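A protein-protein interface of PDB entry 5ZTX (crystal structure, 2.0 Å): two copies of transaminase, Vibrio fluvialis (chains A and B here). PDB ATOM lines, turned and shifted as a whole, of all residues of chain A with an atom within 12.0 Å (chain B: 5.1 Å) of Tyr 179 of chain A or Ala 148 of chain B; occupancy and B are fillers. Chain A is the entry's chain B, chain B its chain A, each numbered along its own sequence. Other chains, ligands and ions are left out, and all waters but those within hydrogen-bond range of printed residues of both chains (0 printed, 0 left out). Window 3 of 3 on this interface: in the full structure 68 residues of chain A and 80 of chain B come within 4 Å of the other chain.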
ATOM      1  N   PHE A  33     -34.380 -10.337 -10.814  1.00  0.00           N
ATOM      2  CA  PHE A  33     -35.003 -11.547 -11.279  1.00  0.00           C
ATOM      3  C   PHE A  33     -35.992 -12.002 -10.214  1.00  0.00           C
ATOM      4  O   PHE A  33     -35.600 -12.604  -9.228  1.00  0.00           O
ATOM      5  CB  PHE A  33     -34.010 -12.692 -11.532  1.00  0.00           C
ATOM      6  CG  PHE A  33     -34.712 -13.895 -12.037  1.00  0.00           C
ATOM      7  CD1 PHE A  33     -35.296 -13.866 -13.312  1.00  0.00           C
ATOM      8  CD2 PHE A  33     -34.954 -14.999 -11.206  1.00  0.00           C
ATOM      9  CE1 PHE A  33     -36.031 -14.948 -13.785  1.00  0.00           C
ATOM     10  CE2 PHE A  33     -35.687 -16.079 -11.684  1.00  0.00           C
ATOM     11  CZ  PHE A  33     -36.238 -16.049 -12.962  1.00  0.00           C
ATOM     12  N   TRP A 161     -25.628 -22.711  13.877  1.00  0.00           N
ATOM     13  CA  TRP A 161     -26.214 -22.549  12.529  1.00  0.00           C
ATOM     14  C   TRP A 161     -27.038 -23.795  12.080  1.00  0.00           C
ATOM     15  O   TRP A 161     -26.577 -24.952  12.238  1.00  0.00           O
ATOM     16  CB  TRP A 161     -25.079 -22.339  11.499  1.00  0.00           C
ATOM     17  CG  TRP A 161     -25.617 -22.206  10.131  1.00  0.00           C
ATOM     18  CD1 TRP A 161     -25.996 -21.046   9.490  1.00  0.00           C
ATOM     19  CD2 TRP A 161     -25.900 -23.286   9.234  1.00  0.00           C
ATOM     20  NE1 TRP A 161     -26.516 -21.357   8.253  1.00  0.00           N
ATOM     21  CE2 TRP A 161     -26.466 -22.728   8.081  1.00  0.00           C
ATOM     22  CE3 TRP A 161     -25.700 -24.684   9.302  1.00  0.00           C
ATOM     23  CZ2 TRP A 161     -26.848 -23.512   6.984  1.00  0.00           C
ATOM     24  CZ3 TRP A 161     -26.103 -25.469   8.226  1.00  0.00           C
ATOM     25  CH2 TRP A 161     -26.665 -24.863   7.070  1.00  0.00           C
ATOM     26  N   ASN A 162     -28.186 -23.582  11.446  1.00  0.00           N
ATOM     27  CA  ASN A 162     -28.839 -24.695  10.714  1.00  0.00           C
ATOM     28  C   ASN A 162     -29.617 -24.154   9.505  1.00  0.00           C
ATOM     29  O   ASN A 162     -29.872 -22.970   9.436  1.00  0.00           O
ATOM     30  CB  ASN A 162     -29.717 -25.528  11.684  1.00  0.00           C
ATOM     31  CG  ASN A 162     -30.807 -24.704  12.334  1.00  0.00           C
ATOM     32  OD1 ASN A 162     -30.682 -24.257  13.511  1.00  0.00           O
ATOM     33  ND2 ASN A 162     -31.886 -24.468  11.567  1.00  0.00           N
ATOM     34  N   ALA A 163     -29.912 -25.010   8.532  1.00  0.00           N
ATOM     35  CA  ALA A 163     -30.685 -24.645   7.320  1.00  0.00           C
ATOM     36  C   ALA A 163     -32.182 -24.631   7.651  1.00  0.00           C
ATOM     37  O   ALA A 163     -32.587 -25.277   8.605  1.00  0.00           O
ATOM     38  CB  ALA A 163     -30.399 -25.645   6.211  1.00  0.00           C
ATOM     39  N   TYR A 164     -32.999 -23.920   6.877  1.00  0.00           N
ATOM     40  CA  TYR A 164     -34.464 -23.855   7.132  1.00  0.00           C
ATOM     41  C   TYR A 164     -35.226 -25.114   6.757  1.00  0.00           C
ATOM     42  O   TYR A 164     -35.581 -25.288   5.600  1.00  0.00           O
ATOM     43  CB  TYR A 164     -35.101 -22.617   6.456  1.00  0.00           C
ATOM     44  CG  TYR A 164     -34.798 -21.356   7.238  1.00  0.00           C
ATOM     45  CD1 TYR A 164     -35.354 -21.162   8.527  1.00  0.00           C
ATOM     46  CD2 TYR A 164     -33.914 -20.382   6.739  1.00  0.00           C
ATOM     47  CE1 TYR A 164     -35.067 -20.025   9.283  1.00  0.00           C
ATOM     48  CE2 TYR A 164     -33.615 -19.239   7.492  1.00  0.00           C
ATOM     49  CZ  TYR A 164     -34.195 -19.061   8.761  1.00  0.00           C
ATOM     50  OH  TYR A 164     -33.915 -17.932   9.509  1.00  0.00           O
ATOM     51  N   PRO A 178     -30.658 -29.141  -0.562  1.00  0.00           N
ATOM     52  CA  PRO A 178     -29.221 -29.394  -0.966  1.00  0.00           C
ATOM     53  C   PRO A 178     -28.491 -28.098  -1.432  1.00  0.00           C
ATOM     54  O   PRO A 178     -27.592 -27.582  -0.733  1.00  0.00           O
ATOM     55  CB  PRO A 178     -29.316 -30.460  -2.080  1.00  0.00           C
ATOM     56  CG  PRO A 178     -30.780 -30.526  -2.446  1.00  0.00           C
ATOM     57  CD  PRO A 178     -31.626 -29.954  -1.320  1.00  0.00           C
ATOM     58  N   TYR A 179     -28.915 -27.576  -2.580  1.00  0.00           N
ATOM     59  CA  TYR A 179     -28.799 -26.144  -2.916  1.00  0.00           C
ATOM     60  C   TYR A 179     -29.320 -25.172  -1.817  1.00  0.00           C
ATOM     61  O   TYR A 179     -28.976 -23.966  -1.847  1.00  0.00           O
ATOM     62  CB  TYR A 179     -29.534 -25.848  -4.263  1.00  0.00           C
ATOM     63  CG  TYR A 179     -30.987 -26.336  -4.289  1.00  0.00           C
ATOM     64  CD1 TYR A 179     -31.982 -25.652  -3.571  1.00  0.00           C
ATOM     65  CD2 TYR A 179     -31.351 -27.518  -4.964  1.00  0.00           C
ATOM     66  CE1 TYR A 179     -33.299 -26.100  -3.540  1.00  0.00           C
ATOM     67  CE2 TYR A 179     -32.676 -27.986  -4.949  1.00  0.00           C
ATOM     68  CZ  TYR A 179     -33.650 -27.263  -4.239  1.00  0.00           C
ATOM     69  OH  TYR A 179     -34.979 -27.650  -4.176  1.00  0.00           O
ATOM     70  N   ASN A 180     -30.193 -25.643  -0.909  1.00  0.00           N
ATOM     71  CA  ASN A 180     -30.680 -24.789   0.207  1.00  0.00           C
ATOM     72  C   ASN A 180     -29.666 -24.512   1.328  1.00  0.00           C
ATOM     73  O   ASN A 180     -29.885 -23.643   2.138  1.00  0.00           O
ATOM     74  CB  ASN A 180     -32.007 -25.325   0.780  1.00  0.00           C
ATOM     75  CG  ASN A 180     -33.213 -24.860  -0.038  1.00  0.00           C
ATOM     76  OD1 ASN A 180     -33.334 -23.671  -0.352  1.00  0.00           O
ATOM     77  ND2 ASN A 180     -34.090 -25.794  -0.414  1.00  0.00           N
ATOM     78  N   SER A 181     -28.563 -25.248   1.401  1.00  0.00           N
ATOM     79  CA  SER A 181     -27.561 -24.912   2.384  1.00  0.00           C
ATOM     80  C   SER A 181     -26.222 -24.665   1.677  1.00  0.00           C
ATOM     81  O   SER A 181     -25.251 -25.369   1.946  1.00  0.00           O
ATOM     82  CB  SER A 181     -27.477 -25.985   3.477  1.00  0.00           C
ATOM     83  OG  SER A 181     -26.921 -27.165   2.988  1.00  0.00           O
ATOM     84  N   VAL A 182     -26.194 -23.710   0.748  1.00  0.00           N
ATOM     85  CA  VAL A 182     -24.908 -23.332   0.090  1.00  0.00           C
ATOM     86  C   VAL A 182     -24.547 -21.983   0.664  1.00  0.00           C
ATOM     87  O   VAL A 182     -23.491 -21.830   1.246  1.00  0.00           O
ATOM     88  CB  VAL A 182     -24.966 -23.371  -1.457  1.00  0.00           C
ATOM     89  CG1 VAL A 182     -23.676 -22.888  -2.069  1.00  0.00           C
ATOM     90  CG2 VAL A 182     -25.201 -24.793  -1.936  1.00  0.00           C
ATOM     91  N   PHE A 183     -25.432 -21.006   0.524  1.00  0.00           N
ATOM     92  CA  PHE A 183     -25.031 -19.639   0.899  1.00  0.00           C
ATOM     93  C   PHE A 183     -24.841 -19.408   2.396  1.00  0.00           C
ATOM     94  O   PHE A 183     -23.931 -18.669   2.768  1.00  0.00           O
ATOM     95  CB  PHE A 183     -25.884 -18.599   0.253  1.00  0.00           C
ATOM     96  CG  PHE A 183     -25.663 -18.513  -1.190  1.00  0.00           C
ATOM     97  CD1 PHE A 183     -24.528 -17.854  -1.683  1.00  0.00           C
ATOM     98  CD2 PHE A 183     -26.525 -19.135  -2.071  1.00  0.00           C
ATOM     99  CE1 PHE A 183     -24.268 -17.823  -3.052  1.00  0.00           C
ATOM    100  CE2 PHE A 183     -26.273 -19.075  -3.439  1.00  0.00           C
ATOM    101  CZ  PHE A 183     -25.164 -18.395  -3.928  1.00  0.00           C
ATOM    102  N   GLY A 184     -25.603 -20.098   3.233  1.00  0.00           N
ATOM    103  CA  GLY A 184     -25.373 -20.034   4.683  1.00  0.00           C
ATOM    104  C   GLY A 184     -24.310 -20.940   5.288  1.00  0.00           C
ATOM    105  O   GLY A 184     -23.814 -20.645   6.396  1.00  0.00           O
ATOM    106  N   LEU A 185     -23.964 -22.029   4.589  1.00  0.00           N
ATOM    107  CA  LEU A 185     -23.122 -23.099   5.169  1.00  0.00           C
ATOM    108  C   LEU A 185     -21.822 -22.559   5.776  1.00  0.00           C
ATOM    109  O   LEU A 185     -21.025 -21.934   5.067  1.00  0.00           O
ATOM    110  CB  LEU A 185     -22.815 -24.181   4.120  1.00  0.00           C
ATOM    111  CG  LEU A 185     -22.195 -25.482   4.669  1.00  0.00           C
ATOM    112  CD1 LEU A 185     -23.217 -26.277   5.478  1.00  0.00           C
ATOM    113  CD2 LEU A 185     -21.530 -26.340   3.595  1.00  0.00           C
ATOM    114  N   PRO A 186     -21.588 -22.774   7.108  1.00  0.00           N
ATOM    115  CA  PRO A 186     -20.293 -22.351   7.665  1.00  0.00           C
ATOM    116  C   PRO A 186     -19.113 -23.047   6.989  1.00  0.00           C
ATOM    117  O   PRO A 186     -19.312 -24.029   6.221  1.00  0.00           O
ATOM    118  CB  PRO A 186     -20.346 -22.786   9.148  1.00  0.00           C
ATOM    119  CG  PRO A 186     -21.784 -23.054   9.439  1.00  0.00           C
ATOM    120  CD  PRO A 186     -22.477 -23.362   8.140  1.00  0.00           C
ATOM    121  N   GLY A 409     -45.041 -25.297   3.009  1.00  0.00           N
ATOM    122  CA  GLY A 409     -43.955 -24.472   2.525  1.00  0.00           C
ATOM    123  C   GLY A 409     -44.285 -23.782   1.228  1.00  0.00           C
ATOM    124  O   GLY A 409     -43.941 -22.610   1.045  1.00  0.00           O
ATOM    125  N   ASN A 410     -45.011 -24.489   0.366  1.00  0.00           N
ATOM    126  CA  ASN A 410     -45.462 -23.982  -0.940  1.00  0.00           C
ATOM    127  C   ASN A 410     -46.316 -22.823  -0.844  1.00  0.00           C
ATOM    128  O   ASN A 410     -46.431 -22.102  -1.818  1.00  0.00           O
ATOM    129  CB  ASN A 410     -46.355 -24.982  -1.694  1.00  0.00           C
ATOM    130  CG  ASN A 410     -45.661 -26.264  -1.990  1.00  0.00           C
ATOM    131  OD1 ASN A 410     -44.497 -26.285  -2.397  1.00  0.00           O
ATOM    132  ND2 ASN A 410     -46.361 -27.362  -1.763  1.00  0.00           N
ATOM    133  N   TRP B 143     -21.805 -23.483  -6.869  1.00  0.00           N
ATOM    134  CA  TRP B 143     -22.132 -24.648  -6.032  1.00  0.00           C
ATOM    135  C   TRP B 143     -23.687 -24.781  -6.025  1.00  0.00           C
ATOM    136  O   TRP B 143     -24.270 -25.852  -6.283  1.00  0.00           O
ATOM    137  CB  TRP B 143     -21.594 -24.506  -4.580  1.00  0.00           C
ATOM    138  CG  TRP B 143     -20.109 -24.708  -4.382  1.00  0.00           C
ATOM    139  CD1 TRP B 143     -19.233 -25.253  -5.293  1.00  0.00           C
ATOM    140  CD2 TRP B 143     -19.318 -24.336  -3.245  1.00  0.00           C
ATOM    141  NE1 TRP B 143     -17.972 -25.276  -4.778  1.00  0.00           N
ATOM    142  CE2 TRP B 143     -17.977 -24.702  -3.535  1.00  0.00           C
ATOM    143  CE3 TRP B 143     -19.597 -23.712  -2.021  1.00  0.00           C
ATOM    144  CZ2 TRP B 143     -16.922 -24.491  -2.625  1.00  0.00           C
ATOM    145  CZ3 TRP B 143     -18.535 -23.488  -1.111  1.00  0.00           C
ATOM    146  CH2 TRP B 143     -17.220 -23.892  -1.410  1.00  0.00           C
ATOM    147  N   PHE B 144     -24.329 -23.639  -5.835  1.00  0.00           N
ATOM    148  CA  PHE B 144     -25.738 -23.535  -5.844  1.00  0.00           C
ATOM    149  C   PHE B 144     -26.308 -23.990  -7.187  1.00  0.00           C
ATOM    150  O   PHE B 144     -27.191 -24.812  -7.225  1.00  0.00           O
ATOM    151  CB  PHE B 144     -26.171 -22.108  -5.584  1.00  0.00           C
ATOM    152  CG  PHE B 144     -27.635 -21.880  -5.887  1.00  0.00           C
ATOM    153  CD1 PHE B 144     -28.599 -22.305  -4.998  1.00  0.00           C
ATOM    154  CD2 PHE B 144     -28.036 -21.217  -7.045  1.00  0.00           C
ATOM    155  CE1 PHE B 144     -29.947 -22.159  -5.304  1.00  0.00           C
ATOM    156  CE2 PHE B 144     -29.385 -20.996  -7.315  1.00  0.00           C
ATOM    157  CZ  PHE B 144     -30.336 -21.488  -6.454  1.00  0.00           C
ATOM    158  N   LEU B 145     -25.791 -23.449  -8.276  1.00  0.00           N
ATOM    159  CA  LEU B 145     -26.341 -23.718  -9.575  1.00  0.00           C
ATOM    160  C   LEU B 145     -26.211 -25.220  -9.892  1.00  0.00           C
ATOM    161  O   LEU B 145     -27.220 -25.909 -10.254  1.00  0.00           O
ATOM    162  CB  LEU B 145     -25.620 -22.925 -10.617  1.00  0.00           C
ATOM    163  CG  LEU B 145     -26.040 -23.172 -12.047  1.00  0.00           C
ATOM    164  CD1 LEU B 145     -27.504 -22.791 -12.236  1.00  0.00           C
ATOM    165  CD2 LEU B 145     -25.145 -22.406 -12.987  1.00  0.00           C
ATOM    166  N   HIS B 146     -24.988 -25.717  -9.775  1.00  0.00           N
ATOM    167  CA  HIS B 146     -24.733 -27.146 -10.083  1.00  0.00           C
ATOM    168  C   HIS B 146     -25.646 -28.081  -9.215  1.00  0.00           C
ATOM    169  O   HIS B 146     -26.202 -29.093  -9.703  1.00  0.00           O
ATOM    170  CB  HIS B 146     -23.272 -27.500  -9.857  1.00  0.00           C
ATOM    171  CG  HIS B 146     -22.319 -26.762 -10.742  1.00  0.00           C
ATOM    172  ND1 HIS B 146     -22.502 -26.631 -12.108  1.00  0.00           N
ATOM    173  CD2 HIS B 146     -21.139 -26.179 -10.460  1.00  0.00           C
ATOM    174  CE1 HIS B 146     -21.453 -26.019 -12.628  1.00  0.00           C
ATOM    175  NE2 HIS B 146     -20.627 -25.708 -11.645  1.00  0.00           N
ATOM    176  N   ALA B 147     -25.804 -27.723  -7.968  1.00  0.00           N
ATOM    177  CA  ALA B 147     -26.694 -28.455  -7.086  1.00  0.00           C
ATOM    178  C   ALA B 147     -28.139 -28.436  -7.596  1.00  0.00           C
ATOM    179  O   ALA B 147     -28.759 -29.456  -7.676  1.00  0.00           O
ATOM    180  CB  ALA B 147     -26.597 -27.958  -5.677  1.00  0.00           C
ATOM    181  N   ALA B 148     -28.626 -27.289  -8.023  1.00  0.00           N
ATOM    182  CA  ALA B 148     -29.967 -27.131  -8.513  1.00  0.00           C
ATOM    183  C   ALA B 148     -30.138 -27.857  -9.807  1.00  0.00           C
ATOM    184  O   ALA B 148     -31.226 -28.233 -10.078  1.00  0.00           O
ATOM    185  CB  ALA B 148     -30.320 -25.661  -8.674  1.00  0.00           C
ATOM    186  N   GLU B 149     -29.061 -28.091 -10.569  1.00  0.00           N
ATOM    187  CA  GLU B 149     -29.096 -28.827 -11.837  1.00  0.00           C
ATOM    188  C   GLU B 149     -28.867 -30.352 -11.682  1.00  0.00           C
ATOM    189  O   GLU B 149     -28.599 -31.035 -12.645  1.00  0.00           O
ATOM    190  CB  GLU B 149     -28.086 -28.220 -12.808  1.00  0.00           C
ATOM    191  CG  GLU B 149     -28.461 -26.817 -13.258  1.00  0.00           C
ATOM    192  CD  GLU B 149     -27.488 -26.204 -14.262  1.00  0.00           C
ATOM    193  OE1 GLU B 149     -26.378 -26.714 -14.400  1.00  0.00           O
ATOM    194  OE2 GLU B 149     -27.829 -25.160 -14.885  1.00  0.00           O
ATOM    195  N   GLY B 150     -28.852 -30.843 -10.464  1.00  0.00           N
ATOM    196  CA  GLY B 150     -28.684 -32.269 -10.216  1.00  0.00           C
ATOM    197  C   GLY B 150     -27.266 -32.755 -10.103  1.00  0.00           C
ATOM    198  O   GLY B 150     -27.050 -33.934 -10.194  1.00  0.00           O
ATOM    199  N   ALA B 324     -33.013 -22.126 -12.914  1.00  0.00           N
ATOM    200  CA  ALA B 324     -32.846 -22.853 -11.650  1.00  0.00           C
ATOM    201  C   ALA B 324     -33.700 -22.271 -10.559  1.00  0.00           C
ATOM    202  O   ALA B 324     -34.391 -23.038  -9.864  1.00  0.00           O
ATOM    203  CB  ALA B 324     -31.392 -22.892 -11.202  1.00  0.00           C
ATOM    204  N   ILE B 328     -36.839 -24.234  -8.642  1.00  0.00           N
ATOM    205  CA  ILE B 328     -36.925 -24.493  -7.202  1.00  0.00           C
ATOM    206  C   ILE B 328     -37.938 -23.568  -6.507  1.00  0.00           C
ATOM    207  O   ILE B 328     -38.157 -23.685  -5.301  1.00  0.00           O
ATOM    208  CB  ILE B 328     -35.530 -24.435  -6.505  1.00  0.00           C
ATOM    209  CG1 ILE B 328     -35.103 -23.007  -6.148  1.00  0.00           C
ATOM    210  CG2 ILE B 328     -34.453 -25.130  -7.344  1.00  0.00           C
ATOM    211  CD1 ILE B 328     -33.915 -22.969  -5.192  1.00  0.00           C
ATOM    212  N   GLU B 330     -37.991 -20.590  -5.405  1.00  0.00           N
ATOM    213  CA  GLU B 330     -37.556 -19.696  -4.320  1.00  0.00           C
ATOM    214  C   GLU B 330     -36.167 -19.122  -4.604  1.00  0.00           C
ATOM    215  O   GLU B 330     -35.425 -19.597  -5.460  1.00  0.00           O
ATOM    216  CB  GLU B 330     -37.539 -20.402  -2.964  1.00  0.00           C
ATOM    217  CG  GLU B 330     -36.670 -21.654  -2.923  1.00  0.00           C
ATOM    218  CD  GLU B 330     -36.936 -22.532  -1.703  1.00  0.00           C
ATOM    219  OE1 GLU B 330     -37.560 -22.058  -0.729  1.00  0.00           O
ATOM    220  OE2 GLU B 330     -36.502 -23.700  -1.715  1.00  0.00           O
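No position is printed for both chains.
Printed residues of chain B that touch a printed residue of chain A: Trp 143, Phe 144, Ala 147, Ala 148, Ile 328 and Glu 330.
Hydrophobic or aromatic side chains of chain B that line the printed part of chain A: Trp 143, Phe 144, Ala 147 and Ile 328.
Among the printed residues, no Asp or Glu carboxylate lies within 4 Å of a Lys or Arg side-chain nitrogen of the other chain.
Printed residues of chain B within 4 Å of Val 182 of chain A: Trp 143 and Phe 144.
Of the printed residues of chain B, Phe 183 of chain A touches Phe 144.
Phe 144 of chain B touches three residues of chain A.
No residue of chain A comes within 4 Å of Glu 149 of chain B.
Ile 328 of chain B touches just one residue of chain A: Tyr 179 (3.6 Å).
Of chain A, only Asn 180 comes within 4 Å of Glu 330 of chain B.
The side-chain amide nitrogen (ND2) of Asn 180 of chain A is in hydrogen-bond range of the side-chain carboxylate (OE2) of Glu 330 of chain B, at 3.4 Å.
Phe 144 of chain B touches Tyr 179 of chain A (CD1 to O, 3.6 Å).
CB of Tyr 179 of chain A touches CB of Ala 147 of chain B, at 3.9 Å.
CD2 of Tyr 179 of chain A touches CA of Ala 148 of chain B, at 3.8 Å.
CE1 of Tyr 179 of chain A touches CD1 of Ile 328 of chain B (3.6 Å).
Trp 143 of chain B touches Val 182 of chain A (CB to CG1, 3.6 Å).
N of Phe 144 of chain B touches CG1 of Val 182 of chain A (3.9 Å).
CE2 of Phe 183 of chain A touches CB of Phe 144 of chain B, 3.7 Å away.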
